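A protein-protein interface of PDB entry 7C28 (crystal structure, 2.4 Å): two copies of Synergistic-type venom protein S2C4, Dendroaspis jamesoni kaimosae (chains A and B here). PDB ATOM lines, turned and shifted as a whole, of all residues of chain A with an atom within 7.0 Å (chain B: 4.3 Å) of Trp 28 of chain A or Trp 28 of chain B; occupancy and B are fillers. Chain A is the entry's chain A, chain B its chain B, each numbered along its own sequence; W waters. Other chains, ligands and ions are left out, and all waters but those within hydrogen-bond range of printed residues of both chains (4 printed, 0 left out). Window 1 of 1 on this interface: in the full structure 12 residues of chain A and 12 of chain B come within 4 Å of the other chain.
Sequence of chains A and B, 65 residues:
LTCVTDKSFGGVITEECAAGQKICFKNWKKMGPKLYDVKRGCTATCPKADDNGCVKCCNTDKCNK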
ATOM      1  N   PHE A  25       5.096  15.904 -14.795  1.00  0.00           N
ATOM      2  CA  PHE A  25       6.387  15.233 -14.874  1.00  0.00           C
ATOM      3  C   PHE A  25       6.358  13.875 -14.188  1.00  0.00           C
ATOM      4  O   PHE A  25       5.562  13.627 -13.279  1.00  0.00           O
ATOM      5  CB  PHE A  25       7.517  16.093 -14.261  1.00  0.00           C
ATOM      6  CG  PHE A  25       7.500  16.151 -12.754  1.00  0.00           C
ATOM      7  CD1 PHE A  25       8.158  15.189 -11.992  1.00  0.00           C
ATOM      8  CD2 PHE A  25       6.842  17.178 -12.099  1.00  0.00           C
ATOM      9  CE1 PHE A  25       8.142  15.246 -10.611  1.00  0.00           C
ATOM     10  CE2 PHE A  25       6.824  17.239 -10.717  1.00  0.00           C
ATOM     11  CZ  PHE A  25       7.480  16.270  -9.973  1.00  0.00           C
ATOM     12  N   LYS A  26       7.237  12.995 -14.664  1.00  0.00           N
ATOM     13  CA  LYS A  26       7.650  11.780 -13.978  1.00  0.00           C
ATOM     14  C   LYS A  26       9.163  11.814 -13.814  1.00  0.00           C
ATOM     15  O   LYS A  26       9.878  12.209 -14.738  1.00  0.00           O
ATOM     16  CB  LYS A  26       7.241  10.528 -14.760  1.00  0.00           C
ATOM     17  CG  LYS A  26       5.776  10.466 -15.128  1.00  0.00           C
ATOM     18  CD  LYS A  26       5.496   9.278 -16.023  1.00  0.00           C
ATOM     19  CE  LYS A  26       5.632   7.973 -15.250  1.00  0.00           C
ATOM     20  NZ  LYS A  26       5.097   6.822 -16.026  1.00  0.00           N
ATOM     21  N   ASN A  27       9.656  11.415 -12.640  1.00  0.00           N
ATOM     22  CA  ASN A  27      11.088  11.456 -12.344  1.00  0.00           C
ATOM     23  C   ASN A  27      11.519  10.145 -11.696  1.00  0.00           C
ATOM     24  O   ASN A  27      11.104   9.837 -10.577  1.00  0.00           O
ATOM     25  CB  ASN A  27      11.425  12.640 -11.438  1.00  0.00           C
ATOM     26  CG  ASN A  27      12.908  12.966 -11.430  1.00  0.00           C
ATOM     27  OD1 ASN A  27      13.752  12.106 -11.702  1.00  0.00           O
ATOM     28  ND2 ASN A  27      13.233  14.218 -11.119  1.00  0.00           N
ATOM     29  N   TRP A  28      12.368   9.388 -12.386  1.00  0.00           N
ATOM     30  CA  TRP A  28      12.864   8.108 -11.890  1.00  0.00           C
ATOM     31  C   TRP A  28      14.097   8.361 -11.024  1.00  0.00           C
ATOM     32  O   TRP A  28      15.149   8.759 -11.536  1.00  0.00           O
ATOM     33  CB  TRP A  28      13.196   7.173 -13.052  1.00  0.00           C
ATOM     34  CG  TRP A  28      12.027   6.400 -13.623  1.00  0.00           C
ATOM     35  CD1 TRP A  28      11.696   5.097 -13.368  1.00  0.00           C
ATOM     36  CD2 TRP A  28      11.061   6.878 -14.571  1.00  0.00           C
ATOM     37  NE1 TRP A  28      10.576   4.741 -14.087  1.00  0.00           N
ATOM     38  CE2 TRP A  28      10.169   5.816 -14.833  1.00  0.00           C
ATOM     39  CE3 TRP A  28      10.862   8.101 -15.220  1.00  0.00           C
ATOM     40  CZ2 TRP A  28       9.094   5.944 -15.715  1.00  0.00           C
ATOM     41  CZ3 TRP A  28       9.793   8.226 -16.094  1.00  0.00           C
ATOM     42  CH2 TRP A  28       8.925   7.154 -16.332  1.00  0.00           C
ATOM     43  N   LYS A  29      13.965   8.159  -9.715  1.00  0.00           N
ATOM     44  CA  LYS A  29      15.087   8.257  -8.788  1.00  0.00           C
ATOM     45  C   LYS A  29      15.430   6.870  -8.257  1.00  0.00           C
ATOM     46  O   LYS A  29      14.539   6.122  -7.836  1.00  0.00           O
ATOM     47  CB  LYS A  29      14.777   9.231  -7.646  1.00  0.00           C
ATOM     48  CG  LYS A  29      14.945  10.694  -8.073  1.00  0.00           C
ATOM     49  CD  LYS A  29      14.555  11.700  -6.999  1.00  0.00           C
ATOM     50  CE  LYS A  29      15.349  12.996  -7.164  1.00  0.00           C
ATOM     51  NZ  LYS A  29      15.084  13.667  -8.472  1.00  0.00           N
ATOM     52  N   LYS A  30      16.722   6.532  -8.286  1.00  0.00           N
ATOM     53  CA  LYS A  30      17.172   5.167  -8.035  1.00  0.00           C
ATOM     54  C   LYS A  30      17.274   4.874  -6.542  1.00  0.00           C
ATOM     55  O   LYS A  30      17.920   5.615  -5.797  1.00  0.00           O
ATOM     56  CB  LYS A  30      18.519   4.936  -8.715  1.00  0.00           C
ATOM     57  CG  LYS A  30      18.955   3.488  -8.793  1.00  0.00           C
ATOM     58  CD  LYS A  30      20.241   3.346  -9.602  1.00  0.00           C
ATOM     59  CE  LYS A  30      20.685   1.891  -9.704  1.00  0.00           C
ATOM     60  NZ  LYS A  30      21.803   1.714 -10.675  1.00  0.00           N
ATOM     61  N   TYR A  36      13.162   1.721  -8.545  1.00  0.00           N
ATOM     62  CA  TYR A  36      13.038   3.154  -8.767  1.00  0.00           C
ATOM     63  C   TYR A  36      11.759   3.695  -8.149  1.00  0.00           C
ATOM     64  O   TYR A  36      10.692   3.086  -8.272  1.00  0.00           O
ATOM     65  CB  TYR A  36      13.051   3.488 -10.264  1.00  0.00           C
ATOM     66  CG  TYR A  36      14.402   3.285 -10.902  1.00  0.00           C
ATOM     67  CD1 TYR A  36      15.337   4.310 -10.930  1.00  0.00           C
ATOM     68  CD2 TYR A  36      14.749   2.064 -11.462  1.00  0.00           C
ATOM     69  CE1 TYR A  36      16.568   4.127 -11.501  1.00  0.00           C
ATOM     70  CE2 TYR A  36      15.981   1.873 -12.037  1.00  0.00           C
ATOM     71  CZ  TYR A  36      16.888   2.907 -12.053  1.00  0.00           C
ATOM     72  OH  TYR A  36      18.122   2.723 -12.627  1.00  0.00           O
ATOM     73  N   ASP A  37      11.882   4.832  -7.474  1.00  0.00           N
ATOM     74  CA  ASP A  37      10.742   5.599  -6.997  1.00  0.00           C
ATOM     75  C   ASP A  37      10.451   6.708  -8.002  1.00  0.00           C
ATOM     76  O   ASP A  37      11.318   7.548  -8.275  1.00  0.00           O
ATOM     77  CB  ASP A  37      11.013   6.178  -5.609  1.00  0.00           C
ATOM     78  CG  ASP A  37       9.752   6.661  -4.924  1.00  0.00           C
ATOM     79  OD1 ASP A  37       9.074   5.839  -4.271  1.00  0.00           O
ATOM     80  OD2 ASP A  37       9.436   7.862  -5.033  1.00  0.00           O
ATOM     81  N   VAL A  38       9.247   6.706  -8.562  1.00  0.00           N
ATOM     82  CA  VAL A  38       8.868   7.649  -9.610  1.00  0.00           C
ATOM     83  C   VAL A  38       8.113   8.800  -8.957  1.00  0.00           C
ATOM     84  O   VAL A  38       6.996   8.620  -8.459  1.00  0.00           O
ATOM     85  CB  VAL A  38       8.026   6.980 -10.701  1.00  0.00           C
ATOM     86  CG1 VAL A  38       7.791   7.949 -11.845  1.00  0.00           C
ATOM     87  CG2 VAL A  38       8.718   5.727 -11.200  1.00  0.00           C
ATOM     88  N   LYS A  39       8.712   9.989  -8.967  1.00  0.00           N
ATOM     89  CA  LYS A  39       8.050  11.181  -8.458  1.00  0.00           C
ATOM     90  C   LYS A  39       7.179  11.783  -9.553  1.00  0.00           C
ATOM     91  O   LYS A  39       7.570  11.826 -10.721  1.00  0.00           O
ATOM     92  CB  LYS A  39       9.072  12.211  -7.973  1.00  0.00           C
ATOM     93  CG  LYS A  39      10.075  11.685  -6.951  1.00  0.00           C
ATOM     94  CD  LYS A  39       9.422  11.420  -5.603  1.00  0.00           C
ATOM     95  CE  LYS A  39      10.400  10.782  -4.620  1.00  0.00           C
ATOM     96  NZ  LYS A  39      11.414  11.752  -4.104  1.00  0.00           N
ATOM     97  N   ARG A  40       5.994  12.246  -9.165  1.00  0.00           N
ATOM     98  CA  ARG A  40       5.023  12.788 -10.105  1.00  0.00           C
ATOM     99  C   ARG A  40       4.410  14.060  -9.535  1.00  0.00           C
ATOM    100  O   ARG A  40       4.203  14.172  -8.325  1.00  0.00           O
ATOM    101  CB  ARG A  40       3.921  11.760 -10.414  1.00  0.00           C
ATOM    102  CG  ARG A  40       4.423  10.408 -10.911  1.00  0.00           C
ATOM    103  CD  ARG A  40       3.332   9.359 -10.814  1.00  0.00           C
ATOM    104  NE  ARG A  40       3.508   8.257 -11.761  1.00  0.00           N
ATOM    105  CZ  ARG A  40       3.989   7.058 -11.435  1.00  0.00           C
ATOM    106  NH1 ARG A  40       4.352   6.805 -10.185  1.00  0.00           N
ATOM    107  NH2 ARG A  40       4.110   6.108 -12.356  1.00  0.00           N
ATOM    108  N   ALA A  49      17.115  15.340 -15.086  1.00  0.00           N
ATOM    109  CA  ALA A  49      17.127  14.080 -14.362  1.00  0.00           C
ATOM    110  C   ALA A  49      18.461  13.878 -13.659  1.00  0.00           C
ATOM    111  O   ALA A  49      19.484  14.433 -14.067  1.00  0.00           O
ATOM    112  CB  ALA A  49      16.863  12.910 -15.313  1.00  0.00           C
ATOM    113  N   ASP A  50      18.433  13.103 -12.571  1.00  0.00           N
ATOM    114  CA  ASP A  50      19.673  12.697 -11.922  1.00  0.00           C
ATOM    115  C   ASP A  50      20.519  11.914 -12.907  1.00  0.00           C
ATOM    116  O   ASP A  50      19.997  11.222 -13.782  1.00  0.00           O
ATOM    117  CB  ASP A  50      19.394  11.819 -10.702  1.00  0.00           C
ATOM    118  CG  ASP A  50      18.654  12.553  -9.610  1.00  0.00           C
ATOM    119  OD1 ASP A  50      18.351  13.750  -9.800  1.00  0.00           O
ATOM    120  OD2 ASP A  50      18.367  11.926  -8.567  1.00  0.00           O
ATOM    121  N   ASP A  51      21.839  11.965 -12.709  1.00  0.00           N
ATOM    122  CA  ASP A  51      22.758  11.272 -13.608  1.00  0.00           C
ATOM    123  C   ASP A  51      22.351   9.819 -13.823  1.00  0.00           C
ATOM    124  O   ASP A  51      22.531   9.273 -14.916  1.00  0.00           O
ATOM    125  CB  ASP A  51      24.182  11.347 -13.057  1.00  0.00           C
ATOM    126  CG  ASP A  51      24.851  12.670 -13.351  1.00  0.00           C
ATOM    127  OD1 ASP A  51      24.472  13.325 -14.345  1.00  0.00           O
ATOM    128  OD2 ASP A  51      25.758  13.058 -12.585  1.00  0.00           O
ATOM    129  N   ASN A  52      21.800   9.179 -12.789  1.00  0.00           N
ATOM    130  CA  ASN A  52      21.372   7.788 -12.843  1.00  0.00           C
ATOM    131  C   ASN A  52      19.865   7.635 -13.040  1.00  0.00           C
ATOM    132  O   ASN A  52      19.319   6.562 -12.759  1.00  0.00           O
ATOM    133  CB  ASN A  52      21.809   7.071 -11.566  1.00  0.00           C
ATOM    134  CG  ASN A  52      21.332   7.781 -10.316  1.00  0.00           C
ATOM    135  OD1 ASN A  52      20.151   7.721  -9.964  1.00  0.00           O
ATOM    136  ND2 ASN A  52      22.244   8.478  -9.648  1.00  0.00           N
ATOM    137  N   GLY A  53      19.183   8.688 -13.491  1.00  0.00           N
ATOM    138  CA  GLY A  53      17.737   8.660 -13.624  1.00  0.00           C
ATOM    139  C   GLY A  53      17.164   8.927 -15.003  1.00  0.00           C
ATOM    140  O   GLY A  53      17.847   8.776 -16.020  1.00  0.00           O
ATOM    141  N   CYS A  54      15.898   9.336 -15.038  1.00  0.00           N
ATOM    142  CA  CYS A  54      15.215   9.654 -16.283  1.00  0.00           C
ATOM    143  C   CYS A  54      13.976  10.480 -15.955  1.00  0.00           C
ATOM    144  O   CYS A  54      13.393  10.334 -14.878  1.00  0.00           O
ATOM    145  CB  CYS A  54      14.840   8.360 -17.026  1.00  0.00           C
ATOM    146  SG  CYS A  54      14.437   8.492 -18.792  1.00  0.00           S
ATOM    147  N   VAL A  55      13.583  11.349 -16.887  1.00  0.00           N
ATOM    148  CA  VAL A  55      12.449  12.252 -16.699  1.00  0.00           C
ATOM    149  C   VAL A  55      11.573  12.190 -17.941  1.00  0.00           C
ATOM    150  O   VAL A  55      12.080  12.180 -19.069  1.00  0.00           O
ATOM    151  CB  VAL A  55      12.904  13.707 -16.419  1.00  0.00           C
ATOM    152  CG1 VAL A  55      11.783  14.718 -16.722  1.00  0.00           C
ATOM    153  CG2 VAL A  55      13.369  13.867 -14.974  1.00  0.00           C
ATOM    154  N   LYS A  56      10.259  12.179 -17.741  1.00  0.00           N
ATOM    155  CA  LYS A  56       9.310  12.295 -18.838  1.00  0.00           C
ATOM    156  C   LYS A  56       8.368  13.449 -18.529  1.00  0.00           C
ATOM    157  O   LYS A  56       7.850  13.543 -17.413  1.00  0.00           O
ATOM    158  CB  LYS A  56       8.537  10.988 -19.049  1.00  0.00           C
ATOM    159  CG  LYS A  56       7.275  11.134 -19.893  1.00  0.00           C
ATOM    160  CD  LYS A  56       6.579   9.789 -20.075  1.00  0.00           C
ATOM    161  CE  LYS A  56       5.296   9.931 -20.869  1.00  0.00           C
ATOM    162  NZ  LYS A  56       4.536   8.649 -20.900  1.00  0.00           N
ATOM    163  N   LYS A  65       0.679   9.286 -15.599  1.00  0.00           N
ATOM    164  CA  LYS A  65       0.250   8.126 -14.805  1.00  0.00           C
ATOM    165  C   LYS A  65       1.404   7.237 -14.323  1.00  0.00           C
ATOM    166  O   LYS A  65       2.266   6.828 -15.100  1.00  0.00           O
ATOM    167  CB  LYS A  65      -0.735   7.272 -15.610  1.00  0.00           C
ATOM    168  CG  LYS A  65      -2.101   7.904 -15.807  1.00  0.00           C
ATOM    169  CD  LYS A  65      -2.865   7.204 -16.917  1.00  0.00           C
ATOM    170  CE  LYS A  65      -2.154   7.370 -18.252  1.00  0.00           C
ATOM    171  NZ  LYS A  65      -2.848   6.654 -19.358  1.00  0.00           N
ATOM    172  N   LYS B  26      19.691   4.130 -22.620  1.00  0.00           N
ATOM    173  CA  LYS B  26      19.121   3.440 -21.470  1.00  0.00           C
ATOM    174  C   LYS B  26      17.612   3.374 -21.658  1.00  0.00           C
ATOM    175  O   LYS B  26      16.987   4.374 -22.021  1.00  0.00           O
ATOM    176  CB  LYS B  26      19.427   4.159 -20.148  1.00  0.00           C
ATOM    177  CG  LYS B  26      20.893   4.411 -19.871  1.00  0.00           C
ATOM    178  CD  LYS B  26      21.082   5.249 -18.602  1.00  0.00           C
ATOM    179  CE  LYS B  26      20.828   4.427 -17.337  1.00  0.00           C
ATOM    180  NZ  LYS B  26      21.269   5.126 -16.095  1.00  0.00           N
ATOM    181  N   ASN B  27      17.017   2.214 -21.381  1.00  0.00           N
ATOM    182  CA  ASN B  27      15.587   2.021 -21.598  1.00  0.00           C
ATOM    183  C   ASN B  27      14.955   1.357 -20.383  1.00  0.00           C
ATOM    184  O   ASN B  27      15.264   0.203 -20.070  1.00  0.00           O
ATOM    185  CB  ASN B  27      15.322   1.185 -22.854  1.00  0.00           C
ATOM    186  CG  ASN B  27      13.889   1.318 -23.343  1.00  0.00           C
ATOM    187  OD1 ASN B  27      12.996   1.701 -22.586  1.00  0.00           O
ATOM    188  ND2 ASN B  27      13.664   0.997 -24.608  1.00  0.00           N
ATOM    189  N   TRP B  28      14.047   2.080 -19.725  1.00  0.00           N
ATOM    190  CA  TRP B  28      13.349   1.590 -18.540  1.00  0.00           C
ATOM    191  C   TRP B  28      12.129   0.788 -18.979  1.00  0.00           C
ATOM    192  O   TRP B  28      11.145   1.358 -19.460  1.00  0.00           O
ATOM    193  CB  TRP B  28      12.929   2.750 -17.641  1.00  0.00           C
ATOM    194  CG  TRP B  28      14.022   3.275 -16.765  1.00  0.00           C
ATOM    195  CD1 TRP B  28      14.193   3.030 -15.433  1.00  0.00           C
ATOM    196  CD2 TRP B  28      15.096   4.140 -17.156  1.00  0.00           C
ATOM    197  NE1 TRP B  28      15.310   3.688 -14.972  1.00  0.00           N
ATOM    198  CE2 TRP B  28      15.881   4.375 -16.013  1.00  0.00           C
ATOM    199  CE3 TRP B  28      15.472   4.734 -18.363  1.00  0.00           C
ATOM    200  CZ2 TRP B  28      17.013   5.183 -16.039  1.00  0.00           C
ATOM    201  CZ3 TRP B  28      16.598   5.535 -18.386  1.00  0.00           C
ATOM    202  CH2 TRP B  28      17.353   5.752 -17.232  1.00  0.00           C
ATOM    203  N   LYS B  29      12.175  -0.525 -18.786  1.00  0.00           N
ATOM    204  CA  LYS B  29      11.043  -1.395 -19.069  1.00  0.00           C
ATOM    205  C   LYS B  29      10.445  -1.868 -17.752  1.00  0.00           C
ATOM    206  O   LYS B  29      11.162  -2.361 -16.875  1.00  0.00           O
ATOM    207  CB  LYS B  29      11.469  -2.595 -19.918  1.00  0.00           C
ATOM    208  CG  LYS B  29      11.718  -2.276 -21.384  1.00  0.00           C
ATOM    209  CD  LYS B  29      10.769  -3.047 -22.294  1.00  0.00           C
ATOM    210  CE  LYS B  29      11.005  -2.693 -23.758  1.00  0.00           C
ATOM    211  NZ  LYS B  29      10.119  -3.460 -24.675  1.00  0.00           N
ATOM    212  N   LYS B  30       9.132  -1.729 -17.623  1.00  0.00           N
ATOM    213  CA  LYS B  30       8.481  -1.952 -16.345  1.00  0.00           C
ATOM    214  C   LYS B  30       8.234  -3.438 -16.128  1.00  0.00           C
ATOM    215  O   LYS B  30       7.661  -4.112 -16.990  1.00  0.00           O
ATOM    216  CB  LYS B  30       7.162  -1.182 -16.275  1.00  0.00           C
ATOM    217  CG  LYS B  30       6.536  -1.175 -14.887  1.00  0.00           C
ATOM    218  CD  LYS B  30       5.302  -0.297 -14.822  1.00  0.00           C
ATOM    219  CE  LYS B  30       4.696  -0.316 -13.425  1.00  0.00           C
ATOM    220  NZ  LYS B  30       3.595   0.682 -13.274  1.00  0.00           N
ATOM    221  N   TYR B  36      11.893  -1.838 -12.522  1.00  0.00           N
ATOM    222  CA  TYR B  36      12.157  -1.560 -13.928  1.00  0.00           C
ATOM    223  C   TYR B  36      13.434  -2.267 -14.359  1.00  0.00           C
ATOM    224  O   TYR B  36      14.448  -2.205 -13.657  1.00  0.00           O
ATOM    225  CB  TYR B  36      12.266  -0.048 -14.174  1.00  0.00           C
ATOM    226  CG  TYR B  36      10.979   0.691 -13.886  1.00  0.00           C
ATOM    227  CD1 TYR B  36      10.087   0.997 -14.906  1.00  0.00           C
ATOM    228  CD2 TYR B  36      10.639   1.059 -12.588  1.00  0.00           C
ATOM    229  CE1 TYR B  36       8.902   1.655 -14.645  1.00  0.00           C
ATOM    230  CE2 TYR B  36       9.456   1.718 -12.318  1.00  0.00           C
ATOM    231  CZ  TYR B  36       8.592   2.016 -13.351  1.00  0.00           C
ATOM    232  OH  TYR B  36       7.411   2.675 -13.090  1.00  0.00           O
ATOM    233  N   ASP B  37      13.388  -2.917 -15.520  1.00  0.00           N
ATOM    234  CA  ASP B  37      14.567  -3.517 -16.135  1.00  0.00           C
ATOM    235  C   ASP B  37      15.166  -2.526 -17.127  1.00  0.00           C
ATOM    236  O   ASP B  37      14.517  -2.159 -18.112  1.00  0.00           O
ATOM    237  CB  ASP B  37      14.192  -4.826 -16.830  1.00  0.00           C
ATOM    238  CG  ASP B  37      15.396  -5.705 -17.133  1.00  0.00           C
ATOM    239  OD1 ASP B  37      15.189  -6.909 -17.392  1.00  0.00           O
ATOM    240  OD2 ASP B  37      16.541  -5.202 -17.124  1.00  0.00           O
ATOM    241  N   VAL B  38      16.411  -2.124 -16.885  1.00  0.00           N
ATOM    242  CA  VAL B  38      17.077  -1.070 -17.645  1.00  0.00           C
ATOM    243  C   VAL B  38      17.950  -1.706 -18.716  1.00  0.00           C
ATOM    244  O   VAL B  38      18.953  -2.361 -18.412  1.00  0.00           O
ATOM    245  CB  VAL B  38      17.907  -0.164 -16.730  1.00  0.00           C
ATOM    246  CG1 VAL B  38      18.533   0.971 -17.532  1.00  0.00           C
ATOM    247  CG2 VAL B  38      17.034   0.378 -15.609  1.00  0.00           C
ATOM    248  N   ASN B  52       4.588   3.419 -20.354  1.00  0.00           N
ATOM    249  CA  ASN B  52       4.859   3.419 -18.923  1.00  0.00           C
ATOM    250  C   ASN B  52       6.354   3.428 -18.613  1.00  0.00           C
ATOM    251  O   ASN B  52       6.745   3.153 -17.470  1.00  0.00           O
ATOM    252  CB  ASN B  52       4.167   2.231 -18.247  1.00  0.00           C
ATOM    253  CG  ASN B  52       4.586   0.886 -18.827  1.00  0.00           C
ATOM    254  OD1 ASN B  52       5.567   0.782 -19.566  1.00  0.00           O
ATOM    255  ND2 ASN B  52       3.831  -0.152 -18.499  1.00  0.00           N
ATOM    256  N   GLY B  53       7.190   3.778 -19.596  1.00  0.00           N
ATOM    257  CA  GLY B  53       8.633   3.762 -19.428  1.00  0.00           C
ATOM    258  C   GLY B  53       9.314   5.101 -19.640  1.00  0.00           C
ATOM    259  O   GLY B  53       8.658   6.147 -19.625  1.00  0.00           O
ATOM    260  N   CYS B  54      10.623   5.069 -19.895  1.00  0.00           N
ATOM    261  CA  CYS B  54      11.443   6.256 -20.103  1.00  0.00           C
ATOM    262  C   CYS B  54      12.726   5.828 -20.798  1.00  0.00           C
ATOM    263  O   CYS B  54      13.194   4.700 -20.616  1.00  0.00           O
ATOM    264  CB  CYS B  54      11.774   6.930 -18.760  1.00  0.00           C
ATOM    265  SG  CYS B  54      12.386   8.636 -18.804  1.00  0.00           S
ATOM    266  N   LYS B  56      16.722   7.375 -22.114  1.00  0.00           N
ATOM    267  CA  LYS B  56      17.751   8.399 -22.176  1.00  0.00           C
ATOM    268  C   LYS B  56      18.781   8.038 -23.236  1.00  0.00           C
ATOM    269  O   LYS B  56      19.277   6.909 -23.268  1.00  0.00           O
ATOM    270  CB  LYS B  56      18.444   8.574 -20.839  1.00  0.00           C
ATOM    271  CG  LYS B  56      19.536   9.601 -20.940  1.00  0.00           C
ATOM    272  CD  LYS B  56      20.292   9.746 -19.653  1.00  0.00           C
ATOM    273  CE  LYS B  56      19.395  10.378 -18.614  1.00  0.00           C
ATOM    274  NZ  LYS B  56      20.202  11.121 -17.645  1.00  0.00           N
HETATM  275  O   HOH W   1      11.895  11.283 -21.434  1.00  0.00           O
HETATM  276  O   HOH W   2       5.677   4.015 -15.041  1.00  0.00           O
HETATM  277  O   HOH W   3       6.063   6.428 -18.497  1.00  0.00           O
HETATM  278  O   HOH W   4      20.444   3.706 -13.449  1.00  0.00           O
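Of the 12 printed residues of chain B, 6 touch a printed residue of chain A. Hydrophobic or aromatic side chains of chain B that line the printed part of chain A: Trp 28, Tyr 36 and Val 38. Hydrophobic or aromatic side chains of chain A that line the printed part of chain B: Trp 28, Tyr 36 and Val 38. Among the printed residues, no Asp or Glu carboxylate lies within 4 Å of a Lys or Arg side-chain nitrogen of the other chain.
Trp 28 of chain B touches its own counterpart, Trp 28 of chain A. Trp 28 of chain A touches Tyr 36 of chain B, and with the chains exchanged Tyr 36 of chain A touches Trp 28 of chain B. Gly 53 of chain A touches Lys 56 of chain B, but with the chains exchanged Lys 56 of chain A does not touch Gly 53 of chain B (4.2 Å). Cys 54 of chain B touches its own counterpart, Cys 54 of chain A. Of the 13 pairs that touch across the chains among the printed residues, 10 have their exchanged pair printed and touching as well.
Water W1 bridges O of Val 55 of chain A (2.5 Å) and SG of Cys 54 of chain B (3.8 Å). Water W4 lies within hydrogen-bond range of the side-chain hydroxyl of Tyr 36 of chain A (2.7 Å), the side-chain amino group of Lys 26 of chain B (3.1 Å) and the backbone carbonyl oxygen of Asn 52 of chain A (3.1 Å). Water W3 lies within hydrogen-bond range of NZ of Lys 26 of chain A (2.7 Å), O of Gly 53 of chain B (2.8 Å) and O of Asn 52 of chain B (3.5 Å). Water W2 lies within hydrogen-bond range of the backbone carbonyl oxygen of Asn 52 of chain B, the side-chain hydroxyl of Tyr 36 of chain B and the side-chain amino group of Lys 26 of chain A.
N of Trp 28 of chain A is in hydrogen-bond range of O of Cys 54 of chain A (2.9 Å). NZ of Lys 29 of chain A is in salt-bridge range of OD1 of Asp 50 of chain A (3.5 Å). The backbone NH (N) of Lys 26 of chain B lies within hydrogen-bond range of the backbone carbonyl oxygen (O) of Lys 56 of chain B. O of Cys 54 of chain B sits at hydrogen-bond distance from N of Trp 28 of chain B (2.9 Å).
Among the printed residues, pairs that only touch across the chains: Trp 28 of chain A with Trp 28 of chain B (3.8 Å), Trp 28 of chain A with Tyr 36 of chain B (3.5 Å), Trp 28 of chain A with Gly 53 of chain B (3.5 Å), Trp 28 of chain A with Cys 54 of chain B (3.6 Å), Tyr 36 of chain A with Trp 28 of chain B (3.4 Å), Tyr 36 of chain A with Val 38 of chain B (3.9 Å), Val 38 of chain A with Tyr 36 of chain B (3.8 Å), Asp 50 of chain A with Lys 56 of chain B (3.9 Å), Gly 53 of chain A with Trp 28 of chain B (3.3 Å), Gly 53 of chain A with Lys 56 of chain B (3.4 Å) and Cys 54 of chain A with Trp 28 of chain B (3.6 Å).
SG of Cys 54 of chain A forms a disulfide with SG of Cys 54 of chain B (2.1 Å). The side-chain sulfur (SG) of Cys 54 of chain B lies within hydrogen-bond range of the backbone NH (N) of Val 55 of chain A.
Trp 28 of chain A touches just these residues of chain B: Trp 28 (3.8 Å), Tyr 36 (3.5 Å), Gly 53 (3.5 Å) and Cys 54 (3.6 Å). Of the printed residues of chain B, Val 38 of chain A touches Tyr 36. Of the printed residues of chain B, Gly 53 of chain A touches Trp 28 (3.3 Å) and Lys 56 (3.4 Å). Printed residues of chain B within 4 Å of Val 55 of chain A: Cys 54 (3.5 Å). Of the printed residues of chain A, Tyr 36 of chain B touches Trp 28 and Val 38. Asp 37 of chain B touches none of the printed residues of chain A. The nearest residue of chain B that does not touch Trp 28 of chain A is Asn 52 of chain B (4.05 Å). The nearest residue of chain A that does not touch Trp 28 of chain B is Asn 52 of chain A (4.2 Å). The nearest printed residue of chain A that does not touch Val 38 of chain B is Lys 30 of chain A (7.0 Å).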
